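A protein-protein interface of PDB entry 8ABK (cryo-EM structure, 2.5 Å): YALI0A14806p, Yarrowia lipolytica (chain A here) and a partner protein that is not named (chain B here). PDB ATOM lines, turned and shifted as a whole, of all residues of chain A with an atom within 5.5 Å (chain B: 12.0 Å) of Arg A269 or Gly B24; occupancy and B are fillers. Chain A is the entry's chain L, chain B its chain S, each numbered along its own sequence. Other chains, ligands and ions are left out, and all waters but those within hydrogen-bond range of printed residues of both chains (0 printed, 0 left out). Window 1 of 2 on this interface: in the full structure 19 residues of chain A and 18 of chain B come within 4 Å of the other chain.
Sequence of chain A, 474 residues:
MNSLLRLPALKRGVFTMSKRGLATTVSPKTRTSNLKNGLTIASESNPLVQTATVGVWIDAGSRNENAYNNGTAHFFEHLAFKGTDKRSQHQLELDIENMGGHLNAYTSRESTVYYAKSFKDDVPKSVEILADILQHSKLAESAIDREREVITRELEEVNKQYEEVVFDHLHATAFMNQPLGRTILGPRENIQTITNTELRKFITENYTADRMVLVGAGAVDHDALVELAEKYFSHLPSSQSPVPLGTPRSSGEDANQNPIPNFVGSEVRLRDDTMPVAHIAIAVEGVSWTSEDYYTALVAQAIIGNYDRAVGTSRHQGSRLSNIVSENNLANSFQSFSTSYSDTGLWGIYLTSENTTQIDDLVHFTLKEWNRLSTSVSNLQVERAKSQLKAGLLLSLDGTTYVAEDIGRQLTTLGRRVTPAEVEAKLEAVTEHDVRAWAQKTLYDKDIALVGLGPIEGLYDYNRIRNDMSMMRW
NH1 of Arg A271 lies close to NE2 of Gln B19.
The backbone NH of Glu A267 lies within hydrogen-bond range of the backbone carbonyl oxygen of Thr B26, at 2.9 Å.
N of Arg A269 lies within hydrogen-bond range of O of Gly B24.
NH2 of Arg A269 lies within hydrogen-bond range of O of Leu A459, 2.8 Å away.
The side-chain carboxylate (OE1) of Glu A267 sits close to the backbone NH (N) of Tyr A462 (3.2 Å).
O of Val A268 is in hydrogen-bond range of N of Gly A452 (3.0 Å).
The backbone carbonyl oxygen of Gly A452 is in hydrogen-bond range of the backbone NH of Leu A270, 2.8 Å away.
NH2 of Arg A269 sits at hydrogen-bond distance from O of Tyr A460 (2.8 Å).
O of Leu A450 lies within hydrogen-bond range of N of Val A268, at 2.9 Å.
Of the printed residues of chain B, Glu A267 touches Gly B24, Tyr B25 and Thr B26.
Leu A270 touches one residue of chain B.
No residue of chain B comes within 4 Å of Leu A459.
No residue of chain B comes within 4 Å of Asp A461.
Of the printed residues of chain B, Tyr A462 touches Ser B28 (3.5 Å) and Pro B29 (3.9 Å).
Of the printed residues of chain A, Lys B20 touches Arg A271 (3.9 Å).
The nearest residue of chain B that does not touch Arg A269 is Tyr B25 (5.1 Å).
The nearest residue of chain A that does not touch Gly B24 is Leu A270 (5.2 Å).
The nearest printed residue of chain A that does not touch Gln B19 is Leu A270 (7.0 Å).
Among the printed residues, merely in contact across the chains: Glu A267 with Gly B24 (3.8 Å), Glu A267 with Tyr B25 (3.3 Å), Val A268 with Gly B24 (3.4 Å), Val A268 with Tyr B25 (3.8 Å), Arg A269 with Ile B22 (3.7 Å), Arg A269 with Ala B23 (3.3 Å), Leu A270 with Ala B23 (3.5 Å), Arg A271 with Lys B20 (3.9 Å), Arg A271 with Ile B22 (3.9 Å), Tyr A460 with Trp B11 (3.6 Å), Tyr A462 with Ser B28 (3.5 Å) and Tyr A462 with Pro B29 (3.9 Å).
Of the 12 printed residues of chain A, 7 touch a printed residue of chain B.
Printed residues of chain A that touch a printed residue of chain B: Glu A267, Val A268, Arg A269, Leu A270, Arg A271, Tyr A460 and Tyr A462.
Hydrophobic or aromatic side chains of chain A within 4 Å of the printed part of chain B: Val A268, Leu A270, Tyr A460 and Tyr A462.
Printed residues of chain B that touch a printed residue of chain A: Trp B11, Gln B19, Lys B20, Ile B22, Ala B23, Gly B24, Tyr B25, Thr B26, Ser B28 and Pro B29.
Hydrophobic or aromatic side chains of chain B within 4 Å of the printed part of chain A: Trp B11, Ala B23, Tyr B25 and Pro B29.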
ATOM      1  N   GLU A 267     -24.716 -25.995  10.013  1.00  0.00           N
ATOM      2  CA  GLU A 267     -26.018 -25.407  10.267  1.00  0.00           C
ATOM      3  C   GLU A 267     -26.965 -25.722   9.121  1.00  0.00           C
ATOM      4  O   GLU A 267     -26.542 -25.866   7.978  1.00  0.00           O
ATOM      5  CB  GLU A 267     -25.926 -23.915  10.572  1.00  0.00           C
ATOM      6  CG  GLU A 267     -24.976 -23.240   9.641  1.00  0.00           C
ATOM      7  CD  GLU A 267     -25.083 -21.732   9.655  1.00  0.00           C
ATOM      8  OE1 GLU A 267     -25.047 -21.140  10.753  1.00  0.00           O
ATOM      9  OE2 GLU A 267     -25.191 -21.147   8.558  1.00  0.00           O
ATOM     10  N   VAL A 268     -28.241 -25.866   9.472  1.00  0.00           N
ATOM     11  CA  VAL A 268     -29.328 -25.878   8.514  1.00  0.00           C
ATOM     12  C   VAL A 268     -30.209 -24.687   8.856  1.00  0.00           C
ATOM     13  O   VAL A 268     -30.617 -24.540  10.004  1.00  0.00           O
ATOM     14  CB  VAL A 268     -30.135 -27.186   8.607  1.00  0.00           C
ATOM     15  CG1 VAL A 268     -31.257 -27.215   7.590  1.00  0.00           C
ATOM     16  CG2 VAL A 268     -29.267 -28.429   8.482  1.00  0.00           C
ATOM     17  N   ARG A 269     -30.509 -23.845   7.867  1.00  0.00           N
ATOM     18  CA  ARG A 269     -31.444 -22.750   8.080  1.00  0.00           C
ATOM     19  C   ARG A 269     -32.654 -22.990   7.195  1.00  0.00           C
ATOM     20  O   ARG A 269     -32.497 -23.170   5.990  1.00  0.00           O
ATOM     21  CB  ARG A 269     -30.832 -21.416   7.668  1.00  0.00           C
ATOM     22  CG  ARG A 269     -29.581 -21.073   8.457  1.00  0.00           C
ATOM     23  CD  ARG A 269     -28.766 -19.929   7.913  1.00  0.00           C
ATOM     24  NE  ARG A 269     -28.929 -18.959   8.973  1.00  0.00           N
ATOM     25  CZ  ARG A 269     -28.099 -18.714   9.978  1.00  0.00           C
ATOM     26  NH1 ARG A 269     -26.899 -19.259  10.086  1.00  0.00           N
ATOM     27  NH2 ARG A 269     -28.496 -17.823  10.860  1.00  0.00           N
ATOM     28  N   LEU A 270     -33.842 -23.016   7.799  1.00  0.00           N
ATOM     29  CA  LEU A 270     -35.072 -23.222   7.056  1.00  0.00           C
ATOM     30  C   LEU A 270     -35.916 -21.988   7.297  1.00  0.00           C
ATOM     31  O   LEU A 270     -36.817 -21.991   8.124  1.00  0.00           O
ATOM     32  CB  LEU A 270     -35.768 -24.485   7.567  1.00  0.00           C
ATOM     33  CG  LEU A 270     -34.898 -25.742   7.580  1.00  0.00           C
ATOM     34  CD1 LEU A 270     -35.428 -26.790   8.550  1.00  0.00           C
ATOM     35  CD2 LEU A 270     -34.752 -26.318   6.179  1.00  0.00           C
ATOM     36  N   ARG A 271     -35.530 -20.904   6.649  1.00  0.00           N
ATOM     37  CA  ARG A 271     -36.211 -19.670   6.942  1.00  0.00           C
ATOM     38  C   ARG A 271     -37.614 -19.721   6.349  1.00  0.00           C
ATOM     39  O   ARG A 271     -37.807 -20.187   5.230  1.00  0.00           O
ATOM     40  CB  ARG A 271     -35.418 -18.509   6.365  1.00  0.00           C
ATOM     41  CG  ARG A 271     -36.126 -17.178   6.506  1.00  0.00           C
ATOM     42  CD  ARG A 271     -35.080 -16.117   6.343  1.00  0.00           C
ATOM     43  NE  ARG A 271     -35.762 -14.856   6.144  1.00  0.00           N
ATOM     44  CZ  ARG A 271     -35.145 -13.708   5.905  1.00  0.00           C
ATOM     45  NH1 ARG A 271     -33.825 -13.675   5.810  1.00  0.00           N
ATOM     46  NH2 ARG A 271     -35.859 -12.614   5.713  1.00  0.00           N
ATOM     47  N   LEU A 450     -26.452 -26.482  14.386  1.00  0.00           N
ATOM     48  CA  LEU A 450     -27.427 -25.436  14.615  1.00  0.00           C
ATOM     49  C   LEU A 450     -28.531 -25.583  13.585  1.00  0.00           C
ATOM     50  O   LEU A 450     -28.250 -25.680  12.400  1.00  0.00           O
ATOM     51  CB  LEU A 450     -26.669 -24.121  14.438  1.00  0.00           C
ATOM     52  CG  LEU A 450     -27.502 -22.872  14.201  1.00  0.00           C
ATOM     53  CD1 LEU A 450     -28.179 -22.420  15.487  1.00  0.00           C
ATOM     54  CD2 LEU A 450     -26.585 -21.768  13.692  1.00  0.00           C
ATOM     55  N   GLY A 452     -32.218 -23.747  12.434  1.00  0.00           N
ATOM     56  CA  GLY A 452     -33.144 -22.658  12.648  1.00  0.00           C
ATOM     57  C   GLY A 452     -34.325 -22.813  11.707  1.00  0.00           C
ATOM     58  O   GLY A 452     -34.129 -23.090  10.534  1.00  0.00           O
ATOM     59  N   ILE A 456     -36.124 -16.446  11.014  1.00  0.00           N
ATOM     60  CA  ILE A 456     -34.824 -16.515  11.663  1.00  0.00           C
ATOM     61  C   ILE A 456     -33.845 -15.554  11.001  1.00  0.00           C
ATOM     62  O   ILE A 456     -32.636 -15.726  11.122  1.00  0.00           O
ATOM     63  CB  ILE A 456     -34.293 -17.956  11.611  1.00  0.00           C
ATOM     64  CG1 ILE A 456     -34.289 -18.447  10.156  1.00  0.00           C
ATOM     65  CG2 ILE A 456     -35.124 -18.826  12.541  1.00  0.00           C
ATOM     66  CD1 ILE A 456     -33.472 -19.698   9.863  1.00  0.00           C
ATOM     67  N   LEU A 459     -31.172 -14.537  13.167  1.00  0.00           N
ATOM     68  CA  LEU A 459     -30.200 -15.479  13.684  1.00  0.00           C
ATOM     69  C   LEU A 459     -28.896 -15.204  12.943  1.00  0.00           C
ATOM     70  O   LEU A 459     -28.914 -15.220  11.723  1.00  0.00           O
ATOM     71  CB  LEU A 459     -30.744 -16.880  13.410  1.00  0.00           C
ATOM     72  CG  LEU A 459     -29.840 -18.021  13.861  1.00  0.00           C
ATOM     73  CD1 LEU A 459     -29.650 -18.010  15.370  1.00  0.00           C
ATOM     74  CD2 LEU A 459     -30.401 -19.365  13.411  1.00  0.00           C
ATOM     75  N   TYR A 460     -27.794 -14.873  13.638  1.00  0.00           N
ATOM     76  CA  TYR A 460     -26.583 -14.506  12.913  1.00  0.00           C
ATOM     77  C   TYR A 460     -25.974 -15.736  12.258  1.00  0.00           C
ATOM     78  O   TYR A 460     -26.408 -16.854  12.532  1.00  0.00           O
ATOM     79  CB  TYR A 460     -25.534 -13.870  13.823  1.00  0.00           C
ATOM     80  CG  TYR A 460     -25.920 -12.501  14.315  1.00  0.00           C
ATOM     81  CD1 TYR A 460     -26.521 -11.589  13.462  1.00  0.00           C
ATOM     82  CD2 TYR A 460     -25.693 -12.120  15.630  1.00  0.00           C
ATOM     83  CE1 TYR A 460     -26.887 -10.327  13.898  1.00  0.00           C
ATOM     84  CE2 TYR A 460     -26.058 -10.860  16.087  1.00  0.00           C
ATOM     85  CZ  TYR A 460     -26.659  -9.963  15.214  1.00  0.00           C
ATOM     86  OH  TYR A 460     -27.022  -8.717  15.630  1.00  0.00           O
ATOM     87  N   ASP A 461     -24.982 -15.518  11.399  1.00  0.00           N
ATOM     88  CA  ASP A 461     -24.288 -16.571  10.675  1.00  0.00           C
ATOM     89  C   ASP A 461     -23.536 -17.490  11.645  1.00  0.00           C
ATOM     90  O   ASP A 461     -23.381 -17.180  12.829  1.00  0.00           O
ATOM     91  CB  ASP A 461     -23.355 -15.909   9.664  1.00  0.00           C
ATOM     92  CG  ASP A 461     -22.601 -14.758  10.311  1.00  0.00           C
ATOM     93  OD1 ASP A 461     -21.791 -15.049  11.209  1.00  0.00           O
ATOM     94  OD2 ASP A 461     -22.856 -13.576   9.940  1.00  0.00           O
ATOM     95  N   TYR A 462     -23.050 -18.621  11.115  1.00  0.00           N
ATOM     96  CA  TYR A 462     -22.405 -19.639  11.923  1.00  0.00           C
ATOM     97  C   TYR A 462     -21.293 -19.066  12.805  1.00  0.00           C
ATOM     98  O   TYR A 462     -21.272 -19.385  13.986  1.00  0.00           O
ATOM     99  CB  TYR A 462     -21.924 -20.821  11.080  1.00  0.00           C
ATOM    100  CG  TYR A 462     -21.497 -22.000  11.916  1.00  0.00           C
ATOM    101  CD1 TYR A 462     -20.184 -22.106  12.363  1.00  0.00           C
ATOM    102  CD2 TYR A 462     -22.384 -23.010  12.271  1.00  0.00           C
ATOM    103  CE1 TYR A 462     -19.774 -23.161  13.160  1.00  0.00           C
ATOM    104  CE2 TYR A 462     -21.977 -24.088  13.055  1.00  0.00           C
ATOM    105  CZ  TYR A 462     -20.665 -24.165  13.501  1.00  0.00           C
ATOM    106  OH  TYR A 462     -20.216 -25.204  14.273  1.00  0.00           O
ATOM    107  N   TRP B  11     -31.621  -6.268  11.489  1.00  0.00           N
ATOM    108  CA  TRP B  11     -31.822  -7.694  11.699  1.00  0.00           C
ATOM    109  C   TRP B  11     -33.213  -7.990  12.247  1.00  0.00           C
ATOM    110  O   TRP B  11     -33.648  -7.369  13.213  1.00  0.00           O
ATOM    111  CB  TRP B  11     -30.777  -8.180  12.680  1.00  0.00           C
ATOM    112  CG  TRP B  11     -29.389  -7.978  12.177  1.00  0.00           C
ATOM    113  CD1 TRP B  11     -28.479  -7.063  12.621  1.00  0.00           C
ATOM    114  CD2 TRP B  11     -28.742  -8.739  11.141  1.00  0.00           C
ATOM    115  NE1 TRP B  11     -27.301  -7.213  11.937  1.00  0.00           N
ATOM    116  CE2 TRP B  11     -27.431  -8.227  11.021  1.00  0.00           C
ATOM    117  CE3 TRP B  11     -29.135  -9.804  10.314  1.00  0.00           C
ATOM    118  CZ2 TRP B  11     -26.517  -8.741  10.094  1.00  0.00           C
ATOM    119  CZ3 TRP B  11     -28.230 -10.310   9.399  1.00  0.00           C
ATOM    120  CH2 TRP B  11     -26.939  -9.780   9.290  1.00  0.00           C
ATOM    121  N   GLY B  12     -33.891  -8.973  11.645  1.00  0.00           N
ATOM    122  CA  GLY B  12     -35.261  -9.262  12.019  1.00  0.00           C
ATOM    123  C   GLY B  12     -36.277  -8.594  11.095  1.00  0.00           C
ATOM    124  O   GLY B  12     -37.374  -9.122  10.931  1.00  0.00           O
ATOM    125  N   MET B  14     -35.211  -6.793   7.843  1.00  0.00           N
ATOM    126  CA  MET B  14     -34.246  -6.185   6.946  1.00  0.00           C
ATOM    127  C   MET B  14     -34.933  -5.519   5.750  1.00  0.00           C
ATOM    128  O   MET B  14     -34.377  -4.590   5.176  1.00  0.00           O
ATOM    129  CB  MET B  14     -33.237  -7.227   6.460  1.00  0.00           C
ATOM    130  CG  MET B  14     -31.986  -6.627   5.855  1.00  0.00           C
ATOM    131  SD  MET B  14     -31.006  -5.810   7.136  1.00  0.00           S
ATOM    132  CE  MET B  14     -30.598  -7.235   8.145  1.00  0.00           C
ATOM    133  N   GLN B  19     -39.378 -14.720   2.718  1.00  0.00           N
ATOM    134  CA  GLN B  19     -38.612 -15.843   2.220  1.00  0.00           C
ATOM    135  C   GLN B  19     -39.281 -17.116   2.700  1.00  0.00           C
ATOM    136  O   GLN B  19     -39.690 -17.211   3.851  1.00  0.00           O
ATOM    137  CB  GLN B  19     -37.187 -15.769   2.753  1.00  0.00           C
ATOM    138  CG  GLN B  19     -36.505 -14.464   2.395  1.00  0.00           C
ATOM    139  CD  GLN B  19     -35.006 -14.535   2.533  1.00  0.00           C
ATOM    140  OE1 GLN B  19     -34.425 -15.602   2.748  1.00  0.00           O
ATOM    141  NE2 GLN B  19     -34.362 -13.385   2.417  1.00  0.00           N
ATOM    142  N   LYS B  20     -39.407 -18.075   1.794  1.00  0.00           N
ATOM    143  CA  LYS B  20     -39.948 -19.374   2.129  1.00  0.00           C
ATOM    144  C   LYS B  20     -39.423 -20.371   1.105  1.00  0.00           C
ATOM    145  O   LYS B  20     -39.284 -20.036  -0.066  1.00  0.00           O
ATOM    146  CB  LYS B  20     -41.468 -19.292   2.039  1.00  0.00           C
ATOM    147  CG  LYS B  20     -42.202 -20.485   2.600  1.00  0.00           C
ATOM    148  CD  LYS B  20     -43.678 -20.288   2.445  1.00  0.00           C
ATOM    149  CE  LYS B  20     -44.486 -21.413   3.051  1.00  0.00           C
ATOM    150  NZ  LYS B  20     -45.936 -21.180   2.855  1.00  0.00           N
ATOM    151  N   GLY B  21     -39.120 -21.590   1.557  1.00  0.00           N
ATOM    152  CA  GLY B  21     -38.812 -22.683   0.654  1.00  0.00           C
ATOM    153  C   GLY B  21     -37.327 -22.851   0.350  1.00  0.00           C
ATOM    154  O   GLY B  21     -36.965 -23.752  -0.401  1.00  0.00           O
ATOM    155  N   ILE B  22     -36.464 -22.009   0.930  1.00  0.00           N
ATOM    156  CA  ILE B  22     -35.028 -22.165   0.743  1.00  0.00           C
ATOM    157  C   ILE B  22     -34.441 -22.813   1.989  1.00  0.00           C
ATOM    158  O   ILE B  22     -34.597 -22.292   3.086  1.00  0.00           O
ATOM    159  CB  ILE B  22     -34.366 -20.799   0.497  1.00  0.00           C
ATOM    160  CG1 ILE B  22     -35.014 -20.052  -0.664  1.00  0.00           C
ATOM    161  CG2 ILE B  22     -32.860 -20.935   0.314  1.00  0.00           C
ATOM    162  CD1 ILE B  22     -34.658 -18.584  -0.676  1.00  0.00           C
ATOM    163  N   ALA B  23     -33.720 -23.918   1.817  1.00  0.00           N
ATOM    164  CA  ALA B  23     -32.955 -24.449   2.932  1.00  0.00           C
ATOM    165  C   ALA B  23     -31.492 -24.117   2.679  1.00  0.00           C
ATOM    166  O   ALA B  23     -31.009 -24.381   1.583  1.00  0.00           O
ATOM    167  CB  ALA B  23     -33.183 -25.934   3.018  1.00  0.00           C
ATOM    168  N   GLY B  24     -30.793 -23.551   3.668  1.00  0.00           N
ATOM    169  CA  GLY B  24     -29.387 -23.219   3.501  1.00  0.00           C
ATOM    170  C   GLY B  24     -28.541 -24.092   4.412  1.00  0.00           C
ATOM    171  O   GLY B  24     -28.968 -24.397   5.521  1.00  0.00           O
ATOM    172  N   TYR B  25     -27.374 -24.526   3.927  1.00  0.00           N
ATOM    173  CA  TYR B  25     -26.533 -25.429   4.695  1.00  0.00           C
ATOM    174  C   TYR B  25     -25.107 -24.912   4.676  1.00  0.00           C
ATOM    175  O   TYR B  25     -24.679 -24.328   3.685  1.00  0.00           O
ATOM    176  CB  TYR B  25     -26.501 -26.803   4.031  1.00  0.00           C
ATOM    177  CG  TYR B  25     -27.861 -27.418   3.873  1.00  0.00           C
ATOM    178  CD1 TYR B  25     -28.699 -27.030   2.841  1.00  0.00           C
ATOM    179  CD2 TYR B  25     -28.321 -28.359   4.783  1.00  0.00           C
ATOM    180  CE1 TYR B  25     -29.950 -27.607   2.688  1.00  0.00           C
ATOM    181  CE2 TYR B  25     -29.576 -28.930   4.658  1.00  0.00           C
ATOM    182  CZ  TYR B  25     -30.388 -28.551   3.603  1.00  0.00           C
ATOM    183  OH  TYR B  25     -31.623 -29.100   3.470  1.00  0.00           O
ATOM    184  N   THR B  26     -24.364 -25.139   5.760  1.00  0.00           N
ATOM    185  CA  THR B  26     -22.936 -24.886   5.699  1.00  0.00           C
ATOM    186  C   THR B  26     -22.232 -25.603   6.834  1.00  0.00           C
ATOM    187  O   THR B  26     -22.878 -26.120   7.729  1.00  0.00           O
ATOM    188  CB  THR B  26     -22.602 -23.391   5.680  1.00  0.00           C
ATOM    189  OG1 THR B  26     -21.227 -23.327   5.301  1.00  0.00           O
ATOM    190  CG2 THR B  26     -22.831 -22.690   7.000  1.00  0.00           C
ATOM    191  N   ILE B  27     -20.903 -25.607   6.801  1.00  0.00           N
ATOM    192  CA  ILE B  27     -20.151 -26.332   7.807  1.00  0.00           C
ATOM    193  C   ILE B  27     -19.238 -25.351   8.528  1.00  0.00           C
ATOM    194  O   ILE B  27     -18.932 -24.274   8.022  1.00  0.00           O
ATOM    195  CB  ILE B  27     -19.377 -27.499   7.172  1.00  0.00           C
ATOM    196  CG1 ILE B  27     -18.441 -26.972   6.079  1.00  0.00           C
ATOM    197  CG2 ILE B  27     -20.352 -28.554   6.651  1.00  0.00           C
ATOM    198  CD1 ILE B  27     -17.530 -28.010   5.459  1.00  0.00           C
ATOM    199  N   SER B  28     -18.806 -25.770   9.709  1.00  0.00           N
ATOM    200  CA  SER B  28     -17.981 -24.982  10.599  1.00  0.00           C
ATOM    201  C   SER B  28     -16.650 -24.638   9.929  1.00  0.00           C
ATOM    202  O   SER B  28     -16.121 -25.435   9.157  1.00  0.00           O
ATOM    203  CB  SER B  28     -17.763 -25.802  11.822  1.00  0.00           C
ATOM    204  OG  SER B  28     -16.775 -25.217  12.641  1.00  0.00           O
ATOM    205  N   PRO B  29     -16.041 -23.460  10.193  1.00  0.00           N
ATOM    206  CA  PRO B  29     -14.710 -23.172   9.663  1.00  0.00           C
ATOM    207  C   PRO B  29     -13.689 -24.189  10.166  1.00  0.00           C
ATOM    208  O   PRO B  29     -12.738 -24.489   9.458  1.00  0.00           O
ATOM    209  CB  PRO B  29     -14.403 -21.766  10.186  1.00  0.00           C
ATOM    210  CG  PRO B  29     -15.307 -21.604  11.378  1.00  0.00           C
ATOM    211  CD  PRO B  29     -16.567 -22.363  11.018  1.00  0.00           C
